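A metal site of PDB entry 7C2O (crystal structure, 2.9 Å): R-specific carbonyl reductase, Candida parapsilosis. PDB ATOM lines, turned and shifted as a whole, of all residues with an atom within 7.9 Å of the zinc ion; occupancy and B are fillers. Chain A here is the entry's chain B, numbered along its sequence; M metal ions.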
ATOM      1  N   GLY A  46       4.267   8.144  33.814  1.00  0.00           N
ATOM      2  CA  GLY A  46       5.036   7.406  32.843  1.00  0.00           C
ATOM      3  C   GLY A  46       6.526   7.637  32.989  1.00  0.00           C
ATOM      4  O   GLY A  46       6.979   8.677  33.463  1.00  0.00           O
ATOM      5  N   LEU A  47       7.299   6.636  32.577  1.00  0.00           N
ATOM      6  CA  LEU A  47       8.763   6.692  32.643  1.00  0.00           C
ATOM      7  C   LEU A  47       9.291   7.289  31.341  1.00  0.00           C
ATOM      8  O   LEU A  47       9.315   6.605  30.314  1.00  0.00           O
ATOM      9  CB  LEU A  47       9.353   5.306  32.896  1.00  0.00           C
ATOM     10  CG  LEU A  47      10.730   5.227  33.565  1.00  0.00           C
ATOM     11  CD1 LEU A  47      10.961   3.836  34.122  1.00  0.00           C
ATOM     12  CD2 LEU A  47      11.854   5.603  32.614  1.00  0.00           C
ATOM     13  N   CYS A  48       9.723   8.532  31.396  1.00  0.00           N
ATOM     14  CA  CYS A  48      10.352   9.176  30.257  1.00  0.00           C
ATOM     15  C   CYS A  48      11.853   8.885  30.250  1.00  0.00           C
ATOM     16  O   CYS A  48      12.470   8.702  31.291  1.00  0.00           O
ATOM     17  CB  CYS A  48      10.121  10.692  30.291  1.00  0.00           C
ATOM     18  SG  CYS A  48      10.931  11.580  28.952  1.00  0.00           S
ATOM     19  N   TYR A  49      12.428   8.823  29.045  1.00  0.00           N
ATOM     20  CA  TYR A  49      13.849   8.488  28.955  1.00  0.00           C
ATOM     21  C   TYR A  49      14.712   9.596  29.536  1.00  0.00           C
ATOM     22  O   TYR A  49      15.805   9.322  30.045  1.00  0.00           O
ATOM     23  CB  TYR A  49      14.250   8.200  27.513  1.00  0.00           C
ATOM     24  CG  TYR A  49      15.537   7.412  27.427  1.00  0.00           C
ATOM     25  CD1 TYR A  49      15.525   6.033  27.440  1.00  0.00           C
ATOM     26  CD2 TYR A  49      16.768   8.062  27.349  1.00  0.00           C
ATOM     27  CE1 TYR A  49      16.702   5.303  27.364  1.00  0.00           C
ATOM     28  CE2 TYR A  49      17.949   7.345  27.277  1.00  0.00           C
ATOM     29  CZ  TYR A  49      17.907   5.968  27.285  1.00  0.00           C
ATOM     30  OH  TYR A  49      19.075   5.249  27.208  1.00  0.00           O
ATOM     31  N   SER A  50      14.257  10.847  29.465  1.00  0.00           N
ATOM     32  CA  SER A  50      15.001  11.957  30.050  1.00  0.00           C
ATOM     33  C   SER A  50      15.121  11.838  31.557  1.00  0.00           C
ATOM     34  O   SER A  50      15.935  12.542  32.161  1.00  0.00           O
ATOM     35  CB  SER A  50      14.333  13.285  29.679  1.00  0.00           C
ATOM     36  OG  SER A  50      13.959  13.312  28.312  1.00  0.00           O
ATOM     37  N   ASP A  51      14.304  10.988  32.194  1.00  0.00           N
ATOM     38  CA  ASP A  51      14.545  10.646  33.591  1.00  0.00           C
ATOM     39  C   ASP A  51      15.888   9.976  33.757  1.00  0.00           C
ATOM     40  O   ASP A  51      16.612  10.240  34.730  1.00  0.00           O
ATOM     41  CB  ASP A  51      13.429   9.737  34.116  1.00  0.00           C
ATOM     42  CG  ASP A  51      12.044  10.360  33.995  1.00  0.00           C
ATOM     43  OD1 ASP A  51      11.951  11.599  33.909  1.00  0.00           O
ATOM     44  OD2 ASP A  51      11.046   9.607  33.997  1.00  0.00           O
ATOM     45  N   GLY A  70      10.674  12.006  36.824  1.00  0.00           N
ATOM     46  CA  GLY A  70       9.376  11.633  36.301  1.00  0.00           C
ATOM     47  C   GLY A  70       8.515  12.837  36.014  1.00  0.00           C
ATOM     48  O   GLY A  70       8.161  13.594  36.922  1.00  0.00           O
ATOM     49  N   HIS A  71       8.168  13.044  34.740  1.00  0.00           N
ATOM     50  CA  HIS A  71       7.387  14.219  34.373  1.00  0.00           C
ATOM     51  C   HIS A  71       6.270  13.871  33.403  1.00  0.00           C
ATOM     52  O   HIS A  71       5.902  14.692  32.552  1.00  0.00           O
ATOM     53  CB  HIS A  71       8.292  15.303  33.788  1.00  0.00           C
ATOM     54  CG  HIS A  71       9.144  14.842  32.647  1.00  0.00           C
ATOM     55  ND1 HIS A  71      10.398  15.369  32.392  1.00  0.00           N
ATOM     56  CD2 HIS A  71       8.934  13.904  31.695  1.00  0.00           C
ATOM     57  CE1 HIS A  71      10.906  14.775  31.329  1.00  0.00           C
ATOM     58  NE2 HIS A  71      10.039  13.885  30.892  1.00  0.00           N
ATOM     59  N   GLU A  72       5.714  12.661  33.512  1.00  0.00           N
ATOM     60  CA  GLU A  72       4.524  12.286  32.761  1.00  0.00           C
ATOM     61  C   GLU A  72       3.397  12.007  33.748  1.00  0.00           C
ATOM     62  O   GLU A  72       2.860  10.898  33.801  1.00  0.00           O
ATOM     63  CB  GLU A  72       4.806  11.060  31.885  1.00  0.00           C
ATOM     64  CG  GLU A  72       5.998  11.244  30.952  1.00  0.00           C
ATOM     65  CD  GLU A  72       6.038  10.228  29.821  1.00  0.00           C
ATOM     66  OE1 GLU A  72       5.550   9.090  30.009  1.00  0.00           O
ATOM     67  OE2 GLU A  72       6.578  10.560  28.736  1.00  0.00           O
ATOM     68  N   GLY A  96       3.246  17.964  32.730  1.00  0.00           N
ATOM     69  CA  GLY A  96       4.274  17.582  31.781  1.00  0.00           C
ATOM     70  C   GLY A  96       5.686  17.690  32.321  1.00  0.00           C
ATOM     71  O   GLY A  96       5.926  17.424  33.510  1.00  0.00           O
ATOM     72  N   ALA A  97       6.633  18.089  31.460  1.00  0.00           N
ATOM     73  CA  ALA A  97       8.042  18.177  31.838  1.00  0.00           C
ATOM     74  C   ALA A  97       8.460  19.576  32.287  1.00  0.00           C
ATOM     75  O   ALA A  97       9.601  19.753  32.719  1.00  0.00           O
ATOM     76  CB  ALA A  97       8.932  17.726  30.677  1.00  0.00           C
ATOM     77  N   TYR A 123      11.431  18.511  37.258  1.00  0.00           N
ATOM     78  CA  TYR A 123      12.395  18.004  38.221  1.00  0.00           C
ATOM     79  C   TYR A 123      13.776  18.565  37.910  1.00  0.00           C
ATOM     80  O   TYR A 123      14.079  18.907  36.756  1.00  0.00           O
ATOM     81  CB  TYR A 123      12.441  16.460  38.247  1.00  0.00           C
ATOM     82  CG  TYR A 123      12.719  15.794  36.915  1.00  0.00           C
ATOM     83  CD1 TYR A 123      13.999  15.780  36.372  1.00  0.00           C
ATOM     84  CD2 TYR A 123      11.702  15.170  36.201  1.00  0.00           C
ATOM     85  CE1 TYR A 123      14.253  15.170  35.160  1.00  0.00           C
ATOM     86  CE2 TYR A 123      11.948  14.554  34.991  1.00  0.00           C
ATOM     87  CZ  TYR A 123      13.233  14.556  34.466  1.00  0.00           C
ATOM     88  OH  TYR A 123      13.496  13.955  33.266  1.00  0.00           O
ATOM     89  N   PRO A 164       1.735   8.980  29.269  1.00  0.00           N
ATOM     90  CA  PRO A 164       2.812   9.162  28.295  1.00  0.00           C
ATOM     91  C   PRO A 164       2.582  10.307  27.324  1.00  0.00           C
ATOM     92  O   PRO A 164       3.549  10.782  26.705  1.00  0.00           O
ATOM     93  CB  PRO A 164       2.867   7.812  27.565  1.00  0.00           C
ATOM     94  CG  PRO A 164       2.261   6.849  28.524  1.00  0.00           C
ATOM     95  CD  PRO A 164       1.179   7.612  29.211  1.00  0.00           C
ATOM     96  N   MET A 166       1.690  13.260  28.289  1.00  0.00           N
ATOM     97  CA  MET A 166       2.041  14.501  28.980  1.00  0.00           C
ATOM     98  C   MET A 166       3.439  14.994  28.626  1.00  0.00           C
ATOM     99  O   MET A 166       3.757  16.149  28.909  1.00  0.00           O
ATOM    100  CB  MET A 166       1.924  14.301  30.492  1.00  0.00           C
ATOM    101  CG  MET A 166       0.499  14.098  30.976  1.00  0.00           C
ATOM    102  SD  MET A 166      -0.556  15.519  30.625  1.00  0.00           S
ATOM    103  CE  MET A 166      -1.559  14.872  29.295  1.00  0.00           C
ATOM    104  N   CYS A 167       4.273  14.149  28.039  1.00  0.00           N
ATOM    105  CA  CYS A 167       5.601  14.563  27.630  1.00  0.00           C
ATOM    106  C   CYS A 167       5.951  13.966  26.282  1.00  0.00           C
ATOM    107  O   CYS A 167       6.134  14.694  25.301  1.00  0.00           O
ATOM    108  CB  CYS A 167       6.645  14.148  28.673  1.00  0.00           C
ATOM    109  SG  CYS A 167       8.331  14.503  28.151  1.00  0.00           S
ATOM    110  N   ALA A 168       6.008  12.632  26.205  1.00  0.00           N
ATOM    111  CA  ALA A 168       6.364  11.980  24.958  1.00  0.00           C
ATOM    112  C   ALA A 168       5.405  12.363  23.841  1.00  0.00           C
ATOM    113  O   ALA A 168       5.824  12.650  22.712  1.00  0.00           O
ATOM    114  CB  ALA A 168       6.397  10.462  25.146  1.00  0.00           C
ATOM    115  N   ILE A 170       3.313  15.127  23.581  1.00  0.00           N
ATOM    116  CA  ILE A 170       3.429  16.527  23.210  1.00  0.00           C
ATOM    117  C   ILE A 170       4.792  16.845  22.601  1.00  0.00           C
ATOM    118  O   ILE A 170       4.911  17.806  21.825  1.00  0.00           O
ATOM    119  CB  ILE A 170       3.131  17.438  24.426  1.00  0.00           C
ATOM    120  CG1 ILE A 170       3.007  18.905  24.002  1.00  0.00           C
ATOM    121  CG2 ILE A 170       4.206  17.288  25.497  1.00  0.00           C
ATOM    122  CD1 ILE A 170       1.963  19.147  22.928  1.00  0.00           C
ATOM    123  N   THR A 171       5.820  16.060  22.910  1.00  0.00           N
ATOM    124  CA  THR A 171       7.151  16.343  22.372  1.00  0.00           C
ATOM    125  C   THR A 171       7.215  16.075  20.868  1.00  0.00           C
ATOM    126  O   THR A 171       8.002  16.710  20.162  1.00  0.00           O
ATOM    127  CB  THR A 171       8.207  15.511  23.106  1.00  0.00           C
ATOM    128  OG1 THR A 171       8.076  15.716  24.521  1.00  0.00           O
ATOM    129  CG2 THR A 171       9.611  15.923  22.682  1.00  0.00           C
ATOM    130  N   LEU A 197       9.047   7.676  21.901  1.00  0.00           N
ATOM    131  CA  LEU A 197       8.655   8.870  21.151  1.00  0.00           C
ATOM    132  C   LEU A 197       8.204   8.525  19.749  1.00  0.00           C
ATOM    133  O   LEU A 197       7.202   9.066  19.255  1.00  0.00           O
ATOM    134  CB  LEU A 197       9.818   9.862  21.113  1.00  0.00           C
ATOM    135  CG  LEU A 197      10.163  10.578  22.413  1.00  0.00           C
ATOM    136  CD1 LEU A 197      11.575  11.095  22.358  1.00  0.00           C
ATOM    137  CD2 LEU A 197       9.183  11.713  22.665  1.00  0.00           C
ATOM    138  N   GLY A 282      13.882  14.959  21.830  1.00  0.00           N
ATOM    139  CA  GLY A 282      14.331  13.963  22.790  1.00  0.00           C
ATOM    140  C   GLY A 282      15.825  13.773  22.862  1.00  0.00           C
ATOM    141  O   GLY A 282      16.286  12.805  23.478  1.00  0.00           O
ATOM    142  N   LEU A 308      11.382  21.474  21.787  1.00  0.00           N
ATOM    143  CA  LEU A 308      11.237  21.092  23.193  1.00  0.00           C
ATOM    144  C   LEU A 308       9.768  21.222  23.593  1.00  0.00           C
ATOM    145  O   LEU A 308       9.186  22.294  23.445  1.00  0.00           O
ATOM    146  CB  LEU A 308      12.113  21.954  24.089  1.00  0.00           C
ATOM    147  CG  LEU A 308      11.930  21.735  25.596  1.00  0.00           C
ATOM    148  CD1 LEU A 308      12.721  20.520  26.067  1.00  0.00           C
ATOM    149  CD2 LEU A 308      12.295  22.970  26.404  1.00  0.00           C
ATOM    150  N   LEU A 309       9.200  20.131  24.090  1.00  0.00           N
ATOM    151  CA  LEU A 309       7.850  20.083  24.676  1.00  0.00           C
ATOM    152  C   LEU A 309       6.844  20.640  23.661  1.00  0.00           C
ATOM    153  O   LEU A 309       6.995  20.447  22.445  1.00  0.00           O
ATOM    154  CB  LEU A 309       7.861  20.799  26.007  1.00  0.00           C
ATOM    155  CG  LEU A 309       8.870  20.212  26.992  1.00  0.00           C
ATOM    156  CD1 LEU A 309       8.943  21.057  28.264  1.00  0.00           C
ATOM    157  CD2 LEU A 309       8.518  18.767  27.293  1.00  0.00           C
ATOM    158  N   ARG A 356       6.200   2.081  26.423  1.00  0.00           N
ATOM    159  CA  ARG A 356       6.341   3.087  27.467  1.00  0.00           C
ATOM    160  C   ARG A 356       6.000   2.471  28.815  1.00  0.00           C
ATOM    161  O   ARG A 356       4.898   1.940  28.991  1.00  0.00           O
ATOM    162  CB  ARG A 356       5.432   4.289  27.186  1.00  0.00           C
ATOM    163  CG  ARG A 356       6.196   5.571  26.945  1.00  0.00           C
ATOM    164  CD  ARG A 356       7.010   5.974  28.170  1.00  0.00           C
ATOM    165  NE  ARG A 356       7.351   7.397  28.138  1.00  0.00           N
ATOM    166  CZ  ARG A 356       8.372   7.899  27.458  1.00  0.00           C
ATOM    167  NH1 ARG A 356       9.162   7.099  26.755  1.00  0.00           N
ATOM    168  NH2 ARG A 356       8.599   9.206  27.486  1.00  0.00           N
HETATM  169 ZN    ZN M   1      10.363  13.848  28.922  1.00  0.00          ZN
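The backbone NH (N) of Ser 50 sits close to the side-chain sulfur (SG) of Cys 48, at 3.4 Å. SG of Cys 48 lies close to NH2 of Arg 356, 3.6 Å away. N of Cys 48 lies within hydrogen-bond range of OD2 of Asp 51 (3.1 Å). The backbone carbonyl oxygen of Ser 50 lies within hydrogen-bond range of the side-chain hydroxyl of Tyr 123, at 3.0 Å.
Merely in contact with the zinc ion: Ser 50 (3.7 Å).
The zinc ion is bound by NE2 of His 71 (2.0 Å). SG of Cys 167 is bound to the zinc ion (2.3 Å). The zinc ion is bound by the side-chain sulfur (SG) of Cys 48 (2.3 Å).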
